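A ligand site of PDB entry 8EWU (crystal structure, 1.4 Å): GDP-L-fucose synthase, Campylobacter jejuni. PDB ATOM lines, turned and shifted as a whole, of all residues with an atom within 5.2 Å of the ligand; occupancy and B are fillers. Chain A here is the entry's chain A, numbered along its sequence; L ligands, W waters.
O of Leu 330 lies within hydrogen-bond range of O10 of the ligand.
ND2 of Asn 155 is in hydrogen-bond range of O3 of the ligand, at 2.8 Å.
A ring nitrogen (ND1) of His 201 sits at hydrogen-bond distance from an oxygen (O6) of the ligand.
An oxygen (O11) of the ligand is in hydrogen-bond range of the side-chain amino group (NZ) of Lys 209 (2.8 Å).
The backbone carbonyl oxygen (O) of Ala 200 is in hydrogen-bond range of a nitrogen (N4) of the ligand.
The side-chain carboxylate of Asp 331 is in hydrogen-bond range of an oxygen (O9) of the ligand (2.6 Å).
N of Val 202 lies within hydrogen-bond range of O6 of the ligand.
N of Leu 253 lies within hydrogen-bond range of N2 of the ligand, 3.0 Å away.
The guanidinium group (NH2) of Arg 260 is in salt-bridge range of an oxygen (O2) of the ligand, at 2.9 Å.
An oxygen (O10) of the ligand lies close to the backbone carbonyl oxygen (O) of Leu 253.
N of Met 91 sits at hydrogen-bond distance from O5 of the ligand (2.8 Å).
The side-chain amide nitrogen of Gln 94 sits at hydrogen-bond distance from an oxygen (O3) of the ligand, at 2.9 Å.
The backbone carbonyl oxygen (O) of Pro 258 lies within hydrogen-bond range of the backbone NH (N) of Ile 306 (3.0 Å).
NH2 of Arg 260 lies within hydrogen-bond range of OG of Ser 187, 2.9 Å away.
The side-chain carboxylate of Asp 331 is in hydrogen-bond range of the backbone NH of Ser 255 (2.8 Å).
The side-chain amide nitrogen of Asn 155 is in hydrogen-bond range of the side-chain amide oxygen of Gln 94 (2.8 Å).
Gly 90 touches the ligand.
Ala 205 touches the ligand.
Ile 206 touches the ligand (CG2 to N2, 3.6 Å).
CB of Leu 252 touches N2 of the ligand (3.95 Å).
CA of Gly 254 touches O10 of the ligand, at 3.7 Å.
Pro 258 touches the ligand (CG to O9, 3.7 Å).
Ile 306 touches the ligand (CG2 to C6, 3.95 Å).
Hydrophobic or aromatic side chains within 4 Å of the ligand: Met 91, His 201, Val 202, Ala 205, Ile 206, Leu 252, Leu 253, Pro 258 and Ile 306.
Within 4 Å of the ligand: Gly 90, Met 91, Gln 94, Asn 155, Ala 200, His 201, Val 202, Ala 205, Ile 206, Lys 209, Leu 252, Leu 253, Gly 254, Pro 258, Arg 260, Ile 306, Leu 330 and Asp 331.
The nearest printed residue that does not touch the ligand is Lys 336 (4.3 Å).
Water W7 lies within hydrogen-bond range of the side-chain amide oxygen of Asn 155 (2.6 Å), an oxygen (O1) of the ligand (2.7 Å) and the side-chain amino group of Lys 336 (2.8 Å).
Water W1 lies within hydrogen-bond range of O6 of the ligand, OG of Ser 187, ND1 of His 201 and NH2 of Arg 260.
Water W4 lies within hydrogen-bond range of O of Ala 200 (2.8 Å), O of Leu 197 (2.8 Å) and N3 of the ligand (2.9 Å).
Water W5 lies within hydrogen-bond range of the side-chain amino group (NZ) of Lys 336 (2.7 Å) and an oxygen (O2) of the ligand (3.2 Å).
Water W2 lies within hydrogen-bond range of O of Leu 253 (2.7 Å), OD1 of Asp 331 (2.8 Å), O10 of the ligand (3.3 Å) and N of Ser 255 (3.4 Å).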
ATOM      1  N   GLY A  90      -4.929  -1.473  -6.447  1.00  0.00           N
ATOM      2  CA  GLY A  90      -6.105  -0.633  -6.208  1.00  0.00           C
ATOM      3  C   GLY A  90      -5.714   0.825  -6.169  1.00  0.00           C
ATOM      4  O   GLY A  90      -4.553   1.229  -6.408  1.00  0.00           O
ATOM      5  N   MET A  91      -6.727   1.622  -5.878  1.00  0.00           N
ATOM      6  CA  MET A  91      -6.672   3.083  -5.906  1.00  0.00           C
ATOM      7  C   MET A  91      -5.443   3.628  -5.151  1.00  0.00           C
ATOM      8  O   MET A  91      -4.667   4.493  -5.674  1.00  0.00           O
ATOM      9  CB  MET A  91      -7.943   3.589  -5.218  1.00  0.00           C
ATOM     10  CG  MET A  91      -7.924   5.041  -4.995  1.00  0.00           C
ATOM     11  SD  MET A  91      -9.455   5.619  -4.175  1.00  0.00           S
ATOM     12  CE  MET A  91      -9.132   5.089  -2.501  1.00  0.00           C
ATOM     13  N   GLN A  94      -2.288   2.882  -6.960  1.00  0.00           N
ATOM     14  CA  GLN A  94      -2.244   3.710  -8.194  1.00  0.00           C
ATOM     15  C   GLN A  94      -1.847   5.158  -7.871  1.00  0.00           C
ATOM     16  O   GLN A  94      -1.211   5.768  -8.686  1.00  0.00           O
ATOM     17  CB  GLN A  94      -3.625   3.732  -8.837  1.00  0.00           C
ATOM     18  CG  GLN A  94      -3.947   2.405  -9.493  1.00  0.00           C
ATOM     19  CD  GLN A  94      -5.266   2.457 -10.207  1.00  0.00           C
ATOM     20  OE1 GLN A  94      -5.425   3.213 -11.185  1.00  0.00           O
ATOM     21  NE2 GLN A  94      -6.233   1.695  -9.697  1.00  0.00           N
ATOM     22  N   ASN A 155      -6.530   7.077 -12.081  1.00  0.00           N
ATOM     23  CA  ASN A 155      -6.225   5.955 -12.990  1.00  0.00           C
ATOM     24  C   ASN A 155      -5.306   6.355 -14.119  1.00  0.00           C
ATOM     25  O   ASN A 155      -5.055   5.503 -14.984  1.00  0.00           O
ATOM     26  CB  ASN A 155      -7.520   5.448 -13.625  1.00  0.00           C
ATOM     27  CG  ASN A 155      -8.486   4.915 -12.601  1.00  0.00           C
ATOM     28  OD1 ASN A 155      -9.717   5.115 -12.787  1.00  0.00           O
ATOM     29  ND2 ASN A 155      -7.991   4.147 -11.622  1.00  0.00           N
ATOM     30  N   SER A 187     -14.780  -4.067 -13.608  1.00  0.00           N
ATOM     31  CA  SER A 187     -14.123  -4.665 -12.430  1.00  0.00           C
ATOM     32  C   SER A 187     -14.493  -6.151 -12.368  1.00  0.00           C
ATOM     33  O   SER A 187     -15.683  -6.489 -12.551  1.00  0.00           O
ATOM     34  CB  SER A 187     -14.505  -3.968 -11.173  1.00  0.00           C
ATOM     35  OG  SER A 187     -13.974  -2.643 -11.148  1.00  0.00           O
ATOM     36  N   LEU A 197      -4.744  -6.597   1.590  1.00  0.00           N
ATOM     37  CA  LEU A 197      -5.684  -5.535   2.025  1.00  0.00           C
ATOM     38  C   LEU A 197      -5.211  -4.183   1.506  1.00  0.00           C
ATOM     39  O   LEU A 197      -6.087  -3.423   1.208  1.00  0.00           O
ATOM     40  CB  LEU A 197      -5.871  -5.546   3.545  1.00  0.00           C
ATOM     41  CG  LEU A 197      -6.357  -6.880   4.153  1.00  0.00           C
ATOM     42  CD1 LEU A 197      -6.685  -6.704   5.612  1.00  0.00           C
ATOM     43  CD2 LEU A 197      -7.535  -7.484   3.399  1.00  0.00           C
ATOM     44  N   ALA A 200      -5.107  -4.545  -2.945  1.00  0.00           N
ATOM     45  CA  ALA A 200      -6.238  -5.115  -3.685  1.00  0.00           C
ATOM     46  C   ALA A 200      -7.140  -4.017  -4.252  1.00  0.00           C
ATOM     47  O   ALA A 200      -7.337  -2.960  -3.627  1.00  0.00           O
ATOM     48  CB  ALA A 200      -6.997  -6.072  -2.839  1.00  0.00           C
ATOM     49  N   HIS A 201      -7.715  -4.320  -5.405  1.00  0.00           N
ATOM     50  CA  HIS A 201      -8.902  -3.641  -5.981  1.00  0.00           C
ATOM     51  C   HIS A 201     -10.096  -3.739  -5.010  1.00  0.00           C
ATOM     52  O   HIS A 201     -10.066  -4.500  -4.010  1.00  0.00           O
ATOM     53  CB  HIS A 201      -9.214  -4.204  -7.381  1.00  0.00           C
ATOM     54  CG  HIS A 201      -8.367  -3.540  -8.422  1.00  0.00           C
ATOM     55  ND1 HIS A 201      -8.627  -2.225  -8.868  1.00  0.00           N
ATOM     56  CD2 HIS A 201      -7.236  -3.939  -9.061  1.00  0.00           C
ATOM     57  CE1 HIS A 201      -7.703  -1.889  -9.778  1.00  0.00           C
ATOM     58  NE2 HIS A 201      -6.844  -2.942  -9.910  1.00  0.00           N
ATOM     59  N   VAL A 202     -11.131  -2.979  -5.313  1.00  0.00           N
ATOM     60  CA  VAL A 202     -12.229  -2.779  -4.327  1.00  0.00           C
ATOM     61  C   VAL A 202     -12.898  -4.116  -3.961  1.00  0.00           C
ATOM     62  O   VAL A 202     -13.095  -4.350  -2.722  1.00  0.00           O
ATOM     63  CB  VAL A 202     -13.223  -1.698  -4.785  1.00  0.00           C
ATOM     64  CG1 VAL A 202     -13.791  -1.955  -6.151  1.00  0.00           C
ATOM     65  CG2 VAL A 202     -14.321  -1.547  -3.762  1.00  0.00           C
ATOM     66  N   ALA A 205     -10.689  -6.512  -1.943  1.00  0.00           N
ATOM     67  CA  ALA A 205     -10.324  -5.829  -0.681  1.00  0.00           C
ATOM     68  C   ALA A 205     -11.525  -5.895   0.265  1.00  0.00           C
ATOM     69  O   ALA A 205     -11.350  -6.209   1.492  1.00  0.00           O
ATOM     70  CB  ALA A 205      -9.914  -4.388  -0.944  1.00  0.00           C
ATOM     71  N   ILE A 206     -12.704  -5.507  -0.199  1.00  0.00           N
ATOM     72  CA  ILE A 206     -13.827  -5.391   0.780  1.00  0.00           C
ATOM     73  C   ILE A 206     -14.233  -6.811   1.184  1.00  0.00           C
ATOM     74  O   ILE A 206     -14.584  -7.023   2.368  1.00  0.00           O
ATOM     75  CB  ILE A 206     -14.999  -4.534   0.273  1.00  0.00           C
ATOM     76  CG1 ILE A 206     -15.795  -5.167  -0.861  1.00  0.00           C
ATOM     77  CG2 ILE A 206     -14.502  -3.144  -0.076  1.00  0.00           C
ATOM     78  CD1 ILE A 206     -17.034  -4.318  -1.249  1.00  0.00           C
ATOM     79  N   LYS A 209     -11.599  -7.913   3.757  1.00  0.00           N
ATOM     80  CA  LYS A 209     -11.756  -7.092   4.981  1.00  0.00           C
ATOM     81  C   LYS A 209     -12.958  -7.600   5.790  1.00  0.00           C
ATOM     82  O   LYS A 209     -12.849  -7.792   7.035  1.00  0.00           O
ATOM     83  CB  LYS A 209     -11.882  -5.611   4.617  1.00  0.00           C
ATOM     84  CG  LYS A 209     -10.535  -5.042   4.161  1.00  0.00           C
ATOM     85  CD  LYS A 209     -10.587  -3.567   3.764  1.00  0.00           C
ATOM     86  CE  LYS A 209      -9.211  -3.002   3.430  1.00  0.00           C
ATOM     87  NZ  LYS A 209      -9.300  -1.563   3.086  1.00  0.00           N
ATOM     88  N   LEU A 252     -14.219   0.339   5.637  1.00  0.00           N
ATOM     89  CA  LEU A 252     -13.928   0.317   4.182  1.00  0.00           C
ATOM     90  C   LEU A 252     -13.578   1.729   3.731  1.00  0.00           C
ATOM     91  O   LEU A 252     -13.759   2.700   4.547  1.00  0.00           O
ATOM     92  CB  LEU A 252     -15.118  -0.287   3.456  1.00  0.00           C
ATOM     93  CG  LEU A 252     -15.505  -1.698   3.919  1.00  0.00           C
ATOM     94  CD1 LEU A 252     -16.688  -2.239   3.112  1.00  0.00           C
ATOM     95  CD2 LEU A 252     -14.335  -2.674   3.867  1.00  0.00           C
ATOM     96  N   LEU A 253     -13.108   1.867   2.498  1.00  0.00           N
ATOM     97  CA  LEU A 253     -12.550   3.180   2.017  1.00  0.00           C
ATOM     98  C   LEU A 253     -13.655   4.018   1.427  1.00  0.00           C
ATOM     99  O   LEU A 253     -14.519   3.465   0.766  1.00  0.00           O
ATOM    100  CB  LEU A 253     -11.443   2.971   0.962  1.00  0.00           C
ATOM    101  CG  LEU A 253     -10.282   2.092   1.402  1.00  0.00           C
ATOM    102  CD1 LEU A 253      -9.149   2.101   0.379  1.00  0.00           C
ATOM    103  CD2 LEU A 253      -9.754   2.498   2.764  1.00  0.00           C
ATOM    104  N   GLY A 254     -13.579   5.340   1.639  1.00  0.00           N
ATOM    105  CA  GLY A 254     -14.390   6.319   0.938  1.00  0.00           C
ATOM    106  C   GLY A 254     -15.781   6.380   1.542  1.00  0.00           C
ATOM    107  O   GLY A 254     -15.973   5.946   2.683  1.00  0.00           O
ATOM    108  N   SER A 255     -16.719   6.831   0.744  1.00  0.00           N
ATOM    109  CA  SER A 255     -18.129   7.041   1.149  1.00  0.00           C
ATOM    110  C   SER A 255     -18.947   5.778   0.977  1.00  0.00           C
ATOM    111  O   SER A 255     -20.029   5.706   1.570  1.00  0.00           O
ATOM    112  CB  SER A 255     -18.729   8.133   0.345  1.00  0.00           C
ATOM    113  OG  SER A 255     -18.876   7.767  -1.012  1.00  0.00           O
ATOM    114  N   PRO A 258     -19.709   5.316  -4.635  1.00  0.00           N
ATOM    115  CA  PRO A 258     -19.431   5.003  -6.042  1.00  0.00           C
ATOM    116  C   PRO A 258     -20.154   3.756  -6.512  1.00  0.00           C
ATOM    117  O   PRO A 258     -20.211   2.775  -5.768  1.00  0.00           O
ATOM    118  CB  PRO A 258     -17.921   4.838  -6.070  1.00  0.00           C
ATOM    119  CG  PRO A 258     -17.481   5.758  -4.988  1.00  0.00           C
ATOM    120  CD  PRO A 258     -18.491   5.535  -3.861  1.00  0.00           C
ATOM    121  N   ARG A 260     -20.660   0.871  -9.705  1.00  0.00           N
ATOM    122  CA  ARG A 260     -20.126   0.269 -10.920  1.00  0.00           C
ATOM    123  C   ARG A 260     -20.659  -1.140 -11.077  1.00  0.00           C
ATOM    124  O   ARG A 260     -21.285  -1.702 -10.137  1.00  0.00           O
ATOM    125  CB  ARG A 260     -18.591   0.273 -10.879  1.00  0.00           C
ATOM    126  CG  ARG A 260     -18.027  -0.452  -9.688  1.00  0.00           C
ATOM    127  CD  ARG A 260     -16.519  -0.582  -9.757  1.00  0.00           C
ATOM    128  NE  ARG A 260     -15.894   0.704  -9.532  1.00  0.00           N
ATOM    129  CZ  ARG A 260     -14.569   0.897  -9.507  1.00  0.00           C
ATOM    130  NH1 ARG A 260     -14.075   2.092  -9.227  1.00  0.00           N
ATOM    131  NH2 ARG A 260     -13.754  -0.105  -9.779  1.00  0.00           N
ATOM    132  N   ILE A 306     -20.600   0.560  -3.841  1.00  0.00           N
ATOM    133  CA  ILE A 306     -19.639  -0.244  -3.044  1.00  0.00           C
ATOM    134  C   ILE A 306     -20.330  -0.628  -1.730  1.00  0.00           C
ATOM    135  O   ILE A 306     -20.134  -1.740  -1.238  1.00  0.00           O
ATOM    136  CB  ILE A 306     -18.352   0.538  -2.816  1.00  0.00           C
ATOM    137  CG1 ILE A 306     -17.726   0.986  -4.142  1.00  0.00           C
ATOM    138  CG2 ILE A 306     -17.392  -0.271  -1.959  1.00  0.00           C
ATOM    139  CD1 ILE A 306     -17.571  -0.095  -5.162  1.00  0.00           C
ATOM    140  N   PHE A 325     -17.853   3.239   6.550  1.00  0.00           N
ATOM    141  CA  PHE A 325     -17.159   3.783   5.363  1.00  0.00           C
ATOM    142  C   PHE A 325     -16.409   5.033   5.787  1.00  0.00           C
ATOM    143  O   PHE A 325     -17.091   6.014   6.214  1.00  0.00           O
ATOM    144  CB  PHE A 325     -18.121   4.052   4.209  1.00  0.00           C
ATOM    145  CG  PHE A 325     -18.354   2.827   3.367  1.00  0.00           C
ATOM    146  CD1 PHE A 325     -17.502   2.517   2.307  1.00  0.00           C
ATOM    147  CD2 PHE A 325     -19.379   1.959   3.669  1.00  0.00           C
ATOM    148  CE1 PHE A 325     -17.687   1.361   1.577  1.00  0.00           C
ATOM    149  CE2 PHE A 325     -19.558   0.808   2.924  1.00  0.00           C
ATOM    150  CZ  PHE A 325     -18.706   0.502   1.897  1.00  0.00           C
ATOM    151  N   LEU A 330     -10.445   8.645  -0.513  1.00  0.00           N
ATOM    152  CA  LEU A 330     -10.875   9.104  -1.858  1.00  0.00           C
ATOM    153  C   LEU A 330     -11.935   8.179  -2.451  1.00  0.00           C
ATOM    154  O   LEU A 330     -11.830   6.941  -2.298  1.00  0.00           O
ATOM    155  CB  LEU A 330      -9.680   9.138  -2.821  1.00  0.00           C
ATOM    156  CG  LEU A 330      -9.068  10.503  -3.136  1.00  0.00           C
ATOM    157  CD1 LEU A 330      -7.942  10.352  -4.169  1.00  0.00           C
ATOM    158  CD2 LEU A 330     -10.097  11.496  -3.631  1.00  0.00           C
ATOM    159  N   ASP A 331     -12.941   8.809  -3.015  1.00  0.00           N
ATOM    160  CA  ASP A 331     -13.701   8.250  -4.140  1.00  0.00           C
ATOM    161  C   ASP A 331     -13.197   8.982  -5.372  1.00  0.00           C
ATOM    162  O   ASP A 331     -12.738  10.148  -5.265  1.00  0.00           O
ATOM    163  CB  ASP A 331     -15.194   8.338  -3.856  1.00  0.00           C
ATOM    164  CG  ASP A 331     -15.511   7.557  -2.590  1.00  0.00           C
ATOM    165  OD1 ASP A 331     -15.064   6.391  -2.494  1.00  0.00           O
ATOM    166  OD2 ASP A 331     -16.157   8.118  -1.692  1.00  0.00           O
ATOM    167  N   GLY A 332     -13.266   8.291  -6.495  1.00  0.00           N
ATOM    168  CA  GLY A 332     -13.062   8.915  -7.806  1.00  0.00           C
ATOM    169  C   GLY A 332     -14.358   8.989  -8.551  1.00  0.00           C
ATOM    170  O   GLY A 332     -15.255   9.809  -8.194  1.00  0.00           O
ATOM    171  N   LYS A 336     -20.289   4.354 -13.025  1.00  0.00           N
ATOM    172  CA  LYS A 336     -19.852   3.678 -14.275  1.00  0.00           C
ATOM    173  C   LYS A 336     -20.892   2.640 -14.665  1.00  0.00           C
ATOM    174  O   LYS A 336     -21.133   1.707 -13.909  1.00  0.00           O
ATOM    175  CB  LYS A 336     -18.516   2.970 -14.086  1.00  0.00           C
ATOM    176  CG  LYS A 336     -17.375   3.814 -13.595  1.00  0.00           C
ATOM    177  CD  LYS A 336     -16.145   2.952 -13.467  1.00  0.00           C
ATOM    178  CE  LYS A 336     -15.073   3.675 -12.692  1.00  0.00           C
ATOM    179  NZ  LYS A 336     -13.804   2.916 -12.806  1.00  0.00           N
HETATM  180  P1  LIG L   1     -10.275   1.499  -9.583  1.00  0.00           P
HETATM  181  O1  LIG L   1     -11.274   2.617  -9.368  1.00  0.00           O
HETATM  182  O2  LIG L   1     -10.961   0.287 -10.201  1.00  0.00           O
HETATM  183  O3  LIG L   1      -9.078   1.877 -10.430  1.00  0.00           O
HETATM  184  O4  LIG L   1      -9.756   1.225  -8.104  1.00  0.00           O
HETATM  185  P2  LIG L   1     -10.218   0.201  -6.913  1.00  0.00           P
HETATM  186  O5  LIG L   1      -9.271   0.415  -5.837  1.00  0.00           O
HETATM  187  O6  LIG L   1     -10.589  -1.107  -7.492  1.00  0.00           O
HETATM  188  O7  LIG L   1     -11.563   0.982  -6.446  1.00  0.00           O
HETATM  189  C1  LIG L   1     -11.516   2.135  -5.588  1.00  0.00           C
HETATM  190  C2  LIG L   1     -12.907   2.600  -5.143  1.00  0.00           C
HETATM  191  O8  LIG L   1     -13.484   1.616  -4.286  1.00  0.00           O
HETATM  192  C3  LIG L   1     -12.891   3.861  -4.260  1.00  0.00           C
HETATM  193  O9  LIG L   1     -14.098   4.627  -4.147  1.00  0.00           O
HETATM  194  C4  LIG L   1     -12.675   3.407  -2.893  1.00  0.00           C
HETATM  195  O10 LIG L   1     -13.026   4.381  -1.858  1.00  0.00           O
HETATM  196  C5  LIG L   1     -13.556   2.126  -2.966  1.00  0.00           C
HETATM  197  N1  LIG L   1     -13.148   1.244  -1.924  1.00  0.00           N
HETATM  198  C6  LIG L   1     -13.850   1.032  -0.787  1.00  0.00           C
HETATM  199  N2  LIG L   1     -13.258   0.200   0.005  1.00  0.00           N
HETATM  200  C7  LIG L   1     -12.088  -0.151  -0.612  1.00  0.00           C
HETATM  201  C8  LIG L   1     -10.956  -0.998  -0.331  1.00  0.00           C
HETATM  202  O11 LIG L   1     -10.881  -1.600   0.736  1.00  0.00           O
HETATM  203  N3  LIG L   1      -9.975  -1.035  -1.269  1.00  0.00           N
HETATM  204  C9  LIG L   1     -10.004  -0.389  -2.421  1.00  0.00           C
HETATM  205  N4  LIG L   1      -8.908  -0.554  -3.284  1.00  0.00           N
HETATM  206  N5  LIG L   1     -10.998   0.446  -2.765  1.00  0.00           N
HETATM  207  C10 LIG L   1     -12.025   0.542  -1.877  1.00  0.00           C
HETATM  208  O   HOH W   1     -11.735  -2.745  -9.390  1.00  0.00           O
HETATM  209  O   HOH W   2     -16.224   4.172  -1.268  1.00  0.00           O
HETATM  210  O   HOH W   3      -8.817   0.675 -13.016  1.00  0.00           O
HETATM  211  O   HOH W   4      -7.326  -2.185  -0.983  1.00  0.00           O
HETATM  212  O   HOH W   5     -12.052   0.864 -13.132  1.00  0.00           O
HETATM  213  O   HOH W   6     -11.041   4.940  -7.846  1.00  0.00           O
HETATM  214  O   HOH W   7     -11.787   4.245 -11.448  1.00  0.00           O
HETATM  215  O   HOH W   8      -6.790   1.168  -2.394  1.00  0.00           O
